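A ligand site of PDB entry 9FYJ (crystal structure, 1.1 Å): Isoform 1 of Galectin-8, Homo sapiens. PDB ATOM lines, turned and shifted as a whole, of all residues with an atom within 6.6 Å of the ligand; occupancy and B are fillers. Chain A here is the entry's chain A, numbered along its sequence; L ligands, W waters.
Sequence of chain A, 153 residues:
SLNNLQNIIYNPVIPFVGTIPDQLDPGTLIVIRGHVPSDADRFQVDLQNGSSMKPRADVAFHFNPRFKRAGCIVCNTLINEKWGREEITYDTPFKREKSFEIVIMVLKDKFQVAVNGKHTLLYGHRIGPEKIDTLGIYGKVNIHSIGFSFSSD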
ATOM      1  N   PRO A  15      -3.810  -0.699  25.791  1.00  0.00           N
ATOM      2  CA  PRO A  15      -3.689  -2.128  26.058  1.00  0.00           C
ATOM      3  C   PRO A  15      -3.812  -2.463  27.536  1.00  0.00           C
ATOM      4  O   PRO A  15      -3.260  -1.787  28.407  1.00  0.00           O
ATOM      5  CB  PRO A  15      -2.282  -2.440  25.541  1.00  0.00           C
ATOM      6  CG  PRO A  15      -1.527  -1.156  25.704  1.00  0.00           C
ATOM      7  CD  PRO A  15      -2.524  -0.103  25.384  1.00  0.00           C
ATOM      8  N   ARG A  42      -9.142  -3.913  14.122  1.00  0.00           N
ATOM      9  CA  ARG A  42      -9.126  -5.217  14.778  1.00  0.00           C
ATOM     10  C   ARG A  42      -8.937  -4.964  16.262  1.00  0.00           C
ATOM     11  O   ARG A  42      -8.424  -3.912  16.657  1.00  0.00           O
ATOM     12  CB  ARG A  42      -8.010  -6.119  14.259  1.00  0.00           C
ATOM     13  CG  ARG A  42      -6.637  -5.503  14.270  1.00  0.00           C
ATOM     14  CD  ARG A  42      -5.598  -6.501  13.795  1.00  0.00           C
ATOM     15  NE  ARG A  42      -5.268  -7.420  14.869  1.00  0.00           N
ATOM     16  CZ  ARG A  42      -4.617  -8.566  14.705  1.00  0.00           C
ATOM     17  NH1 ARG A  42      -4.378  -9.064  13.496  1.00  0.00           N
ATOM     18  NH2 ARG A  42      -4.161  -9.223  15.767  1.00  0.00           N
ATOM     19  N   GLN A  44      -7.991  -7.770  19.930  1.00  0.00           N
ATOM     20  CA  GLN A  44      -7.820  -9.163  20.313  1.00  0.00           C
ATOM     21  C   GLN A  44      -7.902  -9.304  21.827  1.00  0.00           C
ATOM     22  O   GLN A  44      -7.520  -8.407  22.587  1.00  0.00           O
ATOM     23  CB  GLN A  44      -6.503  -9.722  19.797  1.00  0.00           C
ATOM     24  CG  GLN A  44      -5.278  -9.142  20.463  1.00  0.00           C
ATOM     25  CD  GLN A  44      -4.043  -9.141  19.572  1.00  0.00           C
ATOM     26  OE1 GLN A  44      -4.035  -8.490  18.519  1.00  0.00           O
ATOM     27  NE2 GLN A  44      -3.008  -9.892  19.943  1.00  0.00           N
ATOM     28  N   ASP A  46      -6.364 -12.088  24.412  1.00  0.00           N
ATOM     29  CA  ASP A  46      -5.327 -13.114  24.477  1.00  0.00           C
ATOM     30  C   ASP A  46      -5.254 -13.709  25.870  1.00  0.00           C
ATOM     31  O   ASP A  46      -5.066 -12.989  26.857  1.00  0.00           O
ATOM     32  CB  ASP A  46      -3.973 -12.499  24.115  1.00  0.00           C
ATOM     33  CG  ASP A  46      -3.863 -12.130  22.629  1.00  0.00           C
ATOM     34  OD1 ASP A  46      -4.689 -12.580  21.794  1.00  0.00           O
ATOM     35  OD2 ASP A  46      -2.899 -11.374  22.302  1.00  0.00           O
ATOM     36  N   ARG A  56       8.094 -12.889  23.278  1.00  0.00           N
ATOM     37  CA  ARG A  56       6.668 -12.701  23.476  1.00  0.00           C
ATOM     38  C   ARG A  56       6.026 -13.913  24.123  1.00  0.00           C
ATOM     39  O   ARG A  56       6.213 -15.055  23.673  1.00  0.00           O
ATOM     40  CB  ARG A  56       6.010 -12.442  22.148  1.00  0.00           C
ATOM     41  CG  ARG A  56       4.584 -12.148  22.309  1.00  0.00           C
ATOM     42  CD  ARG A  56       4.089 -11.629  21.077  1.00  0.00           C
ATOM     43  NE  ARG A  56       2.644 -11.504  21.140  1.00  0.00           N
ATOM     44  CZ  ARG A  56       1.917 -11.056  20.144  1.00  0.00           C
ATOM     45  NH1 ARG A  56       2.454 -10.669  19.002  1.00  0.00           N
ATOM     46  NH2 ARG A  56       0.610 -11.022  20.269  1.00  0.00           N
ATOM     47  N   HIS A  62      -5.898 -16.884  21.302  1.00  0.00           N
ATOM     48  CA  HIS A  62      -5.972 -15.574  20.667  1.00  0.00           C
ATOM     49  C   HIS A  62      -7.318 -15.501  19.981  1.00  0.00           C
ATOM     50  O   HIS A  62      -7.597 -16.311  19.098  1.00  0.00           O
ATOM     51  CB  HIS A  62      -4.839 -15.508  19.634  1.00  0.00           C
ATOM     52  CG  HIS A  62      -4.835 -14.317  18.709  1.00  0.00           C
ATOM     53  ND1 HIS A  62      -4.524 -13.043  19.111  1.00  0.00           N
ATOM     54  CD2 HIS A  62      -4.953 -14.261  17.354  1.00  0.00           C
ATOM     55  CE1 HIS A  62      -4.469 -12.248  18.046  1.00  0.00           C
ATOM     56  NE2 HIS A  62      -4.725 -12.973  16.963  1.00  0.00           N
ATOM     57  N   ASN A  64      -9.598 -12.888  17.918  1.00  0.00           N
ATOM     58  CA  ASN A  64      -9.215 -11.682  17.174  1.00  0.00           C
ATOM     59  C   ASN A  64     -10.262 -11.265  16.149  1.00  0.00           C
ATOM     60  O   ASN A  64     -10.164 -11.629  14.955  1.00  0.00           O
ATOM     61  CB  ASN A  64      -7.886 -11.987  16.491  1.00  0.00           C
ATOM     62  CG  ASN A  64      -7.364 -10.899  15.580  1.00  0.00           C
ATOM     63  OD1 ASN A  64      -6.658 -11.221  14.612  1.00  0.00           O
ATOM     64  ND2 ASN A  64      -7.618  -9.639  15.881  1.00  0.00           N
ATOM     65  N   ARG A  66     -11.770  -9.007  13.370  1.00  0.00           N
ATOM     66  CA  ARG A  66     -11.212  -8.154  12.339  1.00  0.00           C
ATOM     67  C   ARG A  66     -12.376  -7.557  11.565  1.00  0.00           C
ATOM     68  O   ARG A  66     -13.354  -8.261  11.293  1.00  0.00           O
ATOM     69  CB  ARG A  66     -10.303  -8.934  11.381  1.00  0.00           C
ATOM     70  CG  ARG A  66      -9.140  -9.575  12.097  1.00  0.00           C
ATOM     71  CD  ARG A  66      -8.280 -10.390  11.156  1.00  0.00           C
ATOM     72  NE  ARG A  66      -7.185 -11.006  11.895  1.00  0.00           N
ATOM     73  CZ  ARG A  66      -6.191 -11.661  11.328  1.00  0.00           C
ATOM     74  NH1 ARG A  66      -6.138 -11.834  10.021  1.00  0.00           N
ATOM     75  NH2 ARG A  66      -5.222 -12.156  12.093  1.00  0.00           N
ATOM     76  N   VAL A  74     -10.617 -14.325  13.831  1.00  0.00           N
ATOM     77  CA  VAL A  74      -9.532 -15.283  13.699  1.00  0.00           C
ATOM     78  C   VAL A  74      -9.170 -15.748  15.100  1.00  0.00           C
ATOM     79  O   VAL A  74      -8.989 -14.920  16.009  1.00  0.00           O
ATOM     80  CB  VAL A  74      -8.311 -14.657  13.008  1.00  0.00           C
ATOM     81  CG1 VAL A  74      -7.151 -15.651  12.975  1.00  0.00           C
ATOM     82  CG2 VAL A  74      -8.677 -14.256  11.586  1.00  0.00           C
ATOM     83  N   CYS A  75      -9.074 -17.058  15.297  1.00  0.00           N
ATOM     84  CA  CYS A  75      -8.539 -17.627  16.529  1.00  0.00           C
ATOM     85  C   CYS A  75      -7.293 -18.450  16.229  1.00  0.00           C
ATOM     86  O   CYS A  75      -7.187 -19.111  15.188  1.00  0.00           O
ATOM     87  CB  CYS A  75      -9.568 -18.484  17.271  1.00  0.00           C
ATOM     88  SG  CYS A  75     -11.015 -17.572  17.816  1.00  0.00           S
ATOM     89  N   ASN A  76      -6.347 -18.391  17.161  1.00  0.00           N
ATOM     90  CA  ASN A  76      -5.088 -19.090  16.963  1.00  0.00           C
ATOM     91  C   ASN A  76      -4.372 -19.221  18.310  1.00  0.00           C
ATOM     92  O   ASN A  76      -4.857 -18.754  19.348  1.00  0.00           O
ATOM     93  CB  ASN A  76      -4.233 -18.371  15.914  1.00  0.00           C
ATOM     94  CG  ASN A  76      -3.259 -19.282  15.163  1.00  0.00           C
ATOM     95  OD1 ASN A  76      -2.999 -20.409  15.559  1.00  0.00           O
ATOM     96  ND2 ASN A  76      -2.735 -18.764  14.058  1.00  0.00           N
ATOM     97  N   THR A  77      -3.190 -19.838  18.264  1.00  0.00           N
ATOM     98  CA  THR A  77      -2.316 -20.064  19.399  1.00  0.00           C
ATOM     99  C   THR A  77      -0.908 -19.685  18.972  1.00  0.00           C
ATOM    100  O   THR A  77      -0.491 -19.991  17.853  1.00  0.00           O
ATOM    101  CB  THR A  77      -2.371 -21.542  19.823  1.00  0.00           C
ATOM    102  OG1 THR A  77      -3.674 -21.860  20.318  1.00  0.00           O
ATOM    103  CG2 THR A  77      -1.290 -21.906  20.841  1.00  0.00           C
ATOM    104  N   TRP A  83       2.936 -18.828  15.266  1.00  0.00           N
ATOM    105  CA  TRP A  83       1.480 -18.975  15.186  1.00  0.00           C
ATOM    106  C   TRP A  83       1.137 -20.311  14.533  1.00  0.00           C
ATOM    107  O   TRP A  83       1.821 -20.753  13.615  1.00  0.00           O
ATOM    108  CB  TRP A  83       0.879 -17.836  14.352  1.00  0.00           C
ATOM    109  CG  TRP A  83       0.879 -16.508  15.036  1.00  0.00           C
ATOM    110  CD1 TRP A  83       1.684 -15.439  14.777  1.00  0.00           C
ATOM    111  CD2 TRP A  83       0.027 -16.121  16.111  1.00  0.00           C
ATOM    112  NE1 TRP A  83       1.376 -14.395  15.632  1.00  0.00           N
ATOM    113  CE2 TRP A  83       0.367 -14.791  16.465  1.00  0.00           C
ATOM    114  CE3 TRP A  83      -0.992 -16.768  16.814  1.00  0.00           C
ATOM    115  CZ2 TRP A  83      -0.273 -14.104  17.497  1.00  0.00           C
ATOM    116  CZ3 TRP A  83      -1.628 -16.078  17.827  1.00  0.00           C
ATOM    117  CH2 TRP A  83      -1.272 -14.763  18.151  1.00  0.00           C
ATOM    118  N   GLY A  84       0.059 -20.932  14.994  1.00  0.00           N
ATOM    119  CA  GLY A  84      -0.416 -22.183  14.433  1.00  0.00           C
ATOM    120  C   GLY A  84      -1.443 -21.983  13.349  1.00  0.00           C
ATOM    121  O   GLY A  84      -1.456 -20.952  12.665  1.00  0.00           O
ATOM    122  N   ARG A  85      -2.315 -22.987  13.186  1.00  0.00           N
ATOM    123  CA  ARG A  85      -3.365 -22.959  12.175  1.00  0.00           C
ATOM    124  C   ARG A  85      -4.455 -21.974  12.588  1.00  0.00           C
ATOM    125  O   ARG A  85      -5.010 -22.083  13.685  1.00  0.00           O
ATOM    126  CB  ARG A  85      -3.983 -24.356  12.061  1.00  0.00           C
ATOM    127  CG  ARG A  85      -5.156 -24.472  11.111  1.00  0.00           C
ATOM    128  CD  ARG A  85      -5.820 -25.849  11.279  1.00  0.00           C
ATOM    129  NE  ARG A  85      -6.783 -25.885  12.387  1.00  0.00           N
ATOM    130  CZ  ARG A  85      -7.445 -26.977  12.760  1.00  0.00           C
ATOM    131  NH1 ARG A  85      -7.292 -28.122  12.119  1.00  0.00           N
ATOM    132  NH2 ARG A  85      -8.240 -26.926  13.827  1.00  0.00           N
ATOM    133  N   GLU A  86      -4.758 -21.027  11.718  1.00  0.00           N
ATOM    134  CA  GLU A  86      -5.873 -20.118  11.971  1.00  0.00           C
ATOM    135  C   GLU A  86      -7.201 -20.840  11.881  1.00  0.00           C
ATOM    136  O   GLU A  86      -7.439 -21.628  10.957  1.00  0.00           O
ATOM    137  CB  GLU A  86      -5.860 -18.960  10.961  1.00  0.00           C
ATOM    138  CG  GLU A  86      -4.667 -18.047  11.158  1.00  0.00           C
ATOM    139  CD  GLU A  86      -4.609 -16.845  10.244  1.00  0.00           C
ATOM    140  OE1 GLU A  86      -5.049 -16.947   9.075  1.00  0.00           O
ATOM    141  OE2 GLU A  86      -4.122 -15.790  10.686  1.00  0.00           O
ATOM    142  N   ILE A 137      -5.727  -7.588  26.463  1.00  0.00           N
ATOM    143  CA  ILE A 137      -6.641  -7.058  25.467  1.00  0.00           C
ATOM    144  C   ILE A 137      -5.942  -5.913  24.749  1.00  0.00           C
ATOM    145  O   ILE A 137      -5.450  -4.989  25.410  1.00  0.00           O
ATOM    146  CB  ILE A 137      -7.991  -6.594  26.057  1.00  0.00           C
ATOM    147  CG1 ILE A 137      -8.651  -7.748  26.811  1.00  0.00           C
ATOM    148  CG2 ILE A 137      -8.869  -6.043  24.937  1.00  0.00           C
ATOM    149  CD1 ILE A 137     -10.016  -7.435  27.407  1.00  0.00           C
ATOM    150  N   TYR A 138      -5.881  -6.002  23.425  1.00  0.00           N
ATOM    151  CA  TYR A 138      -5.090  -5.075  22.620  1.00  0.00           C
ATOM    152  C   TYR A 138      -5.910  -4.647  21.410  1.00  0.00           C
ATOM    153  O   TYR A 138      -6.785  -5.381  20.957  1.00  0.00           O
ATOM    154  CB  TYR A 138      -3.800  -5.729  22.116  1.00  0.00           C
ATOM    155  CG  TYR A 138      -3.044  -6.513  23.171  1.00  0.00           C
ATOM    156  CD1 TYR A 138      -2.169  -5.893  24.028  1.00  0.00           C
ATOM    157  CD2 TYR A 138      -3.176  -7.888  23.288  1.00  0.00           C
ATOM    158  CE1 TYR A 138      -1.487  -6.598  25.000  1.00  0.00           C
ATOM    159  CE2 TYR A 138      -2.487  -8.620  24.257  1.00  0.00           C
ATOM    160  CZ  TYR A 138      -1.650  -7.967  25.122  1.00  0.00           C
ATOM    161  OH  TYR A 138      -0.951  -8.666  26.077  1.00  0.00           O
ATOM    162  N   GLY A 139      -5.563  -3.490  20.858  1.00  0.00           N
ATOM    163  CA  GLY A 139      -6.125  -3.021  19.607  1.00  0.00           C
ATOM    164  C   GLY A 139      -7.186  -1.964  19.810  1.00  0.00           C
ATOM    165  O   GLY A 139      -7.241  -1.281  20.831  1.00  0.00           O
ATOM    166  N   LYS A 140      -8.030  -1.802  18.804  1.00  0.00           N
ATOM    167  CA  LYS A 140      -8.999  -0.707  18.771  1.00  0.00           C
ATOM    168  C   LYS A 140     -10.331  -1.227  19.325  1.00  0.00           C
ATOM    169  O   LYS A 140     -11.180  -1.753  18.608  1.00  0.00           O
ATOM    170  CB  LYS A 140      -9.081  -0.070  17.382  1.00  0.00           C
ATOM    171  CG  LYS A 140      -7.805   0.737  17.024  1.00  0.00           C
ATOM    172  CD  LYS A 140      -7.930   1.599  15.763  1.00  0.00           C
ATOM    173  CE  LYS A 140      -6.573   2.195  15.368  1.00  0.00           C
ATOM    174  NZ  LYS A 140      -6.649   3.063  14.147  1.00  0.00           N
HETATM  175  C1  LIG L   1      -3.351 -14.898  14.015  1.00  0.00           C
HETATM  176  C2  LIG L   1      -2.285 -13.862  13.807  1.00  0.00           C
HETATM  177  O1  LIG L   1      -3.175 -16.044  13.224  1.00  0.00           O
HETATM  178  C3  LIG L   1      -1.375 -12.464  12.096  1.00  0.00           C
HETATM  179  C4  LIG L   1      -0.193 -14.532  10.806  1.00  0.00           C
HETATM  180  O2  LIG L   1      -2.419 -13.373  12.460  1.00  0.00           O
HETATM  181  C5  LIG L   1      -0.957 -16.551   9.079  1.00  0.00           C
HETATM  182  C6  LIG L   1      -0.757 -15.282   8.589  1.00  0.00           C
HETATM  183  C7  LIG L   1      -0.376 -14.264   9.448  1.00  0.00           C
HETATM  184  C8  LIG L   1      -1.314 -11.266  13.038  1.00  0.00           C
HETATM  185  C9  LIG L   1      -0.199  -9.761  11.584  1.00  0.00           C
HETATM  186  C10 LIG L   1      -1.198  -8.705  11.592  1.00  0.00           C
HETATM  187  C11 LIG L   1      -2.042  -7.875  11.574  1.00  0.00           C
HETATM  188  C12 LIG L   1      -1.253 -11.709  14.482  1.00  0.00           C
HETATM  189  C13 LIG L   1      -0.202 -10.123  15.960  1.00  0.00           C
HETATM  190  C14 LIG L   1      -0.477  -9.017  16.912  1.00  0.00           C
HETATM  191  C15 LIG L   1      -0.597  -7.846  18.700  1.00  0.00           C
HETATM  192  C16 LIG L   1      -0.561  -7.354  20.008  1.00  0.00           C
HETATM  193  C17 LIG L   1      -0.886  -6.030  20.234  1.00  0.00           C
HETATM  194  C18 LIG L   1      -1.250  -5.179  19.175  1.00  0.00           C
HETATM  195  C19 LIG L   1      -1.617  -3.747  19.461  1.00  0.00           C
HETATM  196  C20 LIG L   1      -1.286  -5.670  17.868  1.00  0.00           C
HETATM  197  C21 LIG L   1      -0.951  -6.994  17.664  1.00  0.00           C
HETATM  198  C22 LIG L   1      -1.149  -7.316  15.143  1.00  0.00           C
HETATM  199  C23 LIG L   1      -2.377 -12.694  14.779  1.00  0.00           C
HETATM  200  C24 LIG L   1      -0.394 -15.823  11.282  1.00  0.00           C
HETATM  201  C25 LIG L   1      -0.771 -16.816  10.417  1.00  0.00           C
HETATM  202  N1  LIG L   1      -0.298  -9.113  18.222  1.00  0.00           N
HETATM  203  N2  LIG L   1      -0.864  -7.773  16.511  1.00  0.00           N
HETATM  204  O3  LIG L   1      -0.152 -10.470  12.823  1.00  0.00           O
HETATM  205  O4  LIG L   1      -1.411 -10.581  15.345  1.00  0.00           O
HETATM  206  O5  LIG L   1      -1.376  -3.309  20.612  1.00  0.00           O
HETATM  207  O6  LIG L   1      -2.153  -3.087  18.539  1.00  0.00           O
HETATM  208  O7  LIG L   1      -3.625 -11.997  14.672  1.00  0.00           O
HETATM  209  S1  LIG L   1       0.269 -13.247  11.933  1.00  0.00           S
HETATM  210 CL1  LIG L   1      -0.966 -18.427  11.043  1.00  0.00          CL
HETATM  211 CL2  LIG L   1      -1.481 -17.796   7.998  1.00  0.00          CL
HETATM  212  O   HOH W   1      -3.396  -2.110  22.123  1.00  0.00           O
HETATM  213  O   HOH W   2      -3.895 -13.461   9.400  1.00  0.00           O
HETATM  214  O   HOH W   3      -2.775  -0.575  19.161  1.00  0.00           O
HETATM  215  O   HOH W   4       2.718 -10.616  13.478  1.00  0.00           O
HETATM  216  O   HOH W   5      -4.088  -4.039  16.823  1.00  0.00           O
HETATM  217  O   HOH W   6      -2.176 -11.417   8.836  1.00  0.00           O
HETATM  218  O   HOH W   7      -0.840 -21.697   9.825  1.00  0.00           O
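The side-chain amide oxygen (OD1) of Asn 64 lies within hydrogen-bond range of an oxygen (O7) of the ligand (3.1 Å). An oxygen (O1) of the ligand lies within hydrogen-bond range of the side-chain carboxylate (OE2) of Glu 86, 2.7 Å away. An oxygen (O7) of the ligand is in hydrogen-bond range of the guanidinium group of Arg 42. A nitrogen (N1) of the ligand is in hydrogen-bond range of the guanidinium group of Arg 56, 2.9 Å away. The side-chain amide nitrogen of Asn 76 sits at hydrogen-bond distance from an oxygen (O1) of the ligand, 2.9 Å away. A nitrogen (N1) of the ligand lies within hydrogen-bond range of the side-chain amide nitrogen (NE2) of Gln 44 (3.3 Å). NH2 of Arg 66 lies within hydrogen-bond range of O7 of the ligand, 3.0 Å away. A ring nitrogen (NE2) of His 62 lies within hydrogen-bond range of an oxygen (O7) of the ligand (2.7 Å).
The backbone NH (N) of Gln 44 lies within hydrogen-bond range of the backbone carbonyl oxygen (O) of Tyr 138. The guanidinium group (NE) of Arg 66 sits at hydrogen-bond distance from the side-chain amide oxygen (OD1) of Asn 64 (2.8 Å). The backbone NH of Asn 64 lies within hydrogen-bond range of the backbone carbonyl oxygen of Val 74. N of Gly 84 lies within hydrogen-bond range of O of Thr 77 (3.1 Å). OD1 of Asp 46 sits at hydrogen-bond distance from ND1 of His 62, at 2.7 Å. The side-chain amide oxygen (OD1) of Asn 64 sits at hydrogen-bond distance from the guanidinium group (NH1) of Arg 42 (3.3 Å). The backbone carbonyl oxygen (O) of Gly 84 sits at hydrogen-bond distance from the side-chain amide nitrogen (ND2) of Asn 76 (2.9 Å). OD1 of Asn 76 sits close to O of Arg 85, 3.2 Å away.
CZ2 of Trp 83 touches C23 of the ligand (3.7 Å). O of Gly 84 touches CL1 of the ligand, at 3.0 Å. CB of Tyr 138 touches C17 of the ligand, 3.5 Å away. Within 4 Å of the ligand: Arg 42, Gln 44, Arg 56, His 62, Asn 64, Arg 66, Asn 76, Trp 83, Gly 84, Glu 86 and Tyr 138.
Water W1 bridges an oxygen (O5) of the ligand (2.8 Å) and the backbone NH of Gly 139 (2.9 Å). Water W2 lies within hydrogen-bond range of the side-chain carboxylate (OE2) of Glu 86 (2.7 Å), the guanidinium group (NH1) of Arg 66 (2.8 Å) and an oxygen (O2) of the ligand (3.4 Å).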
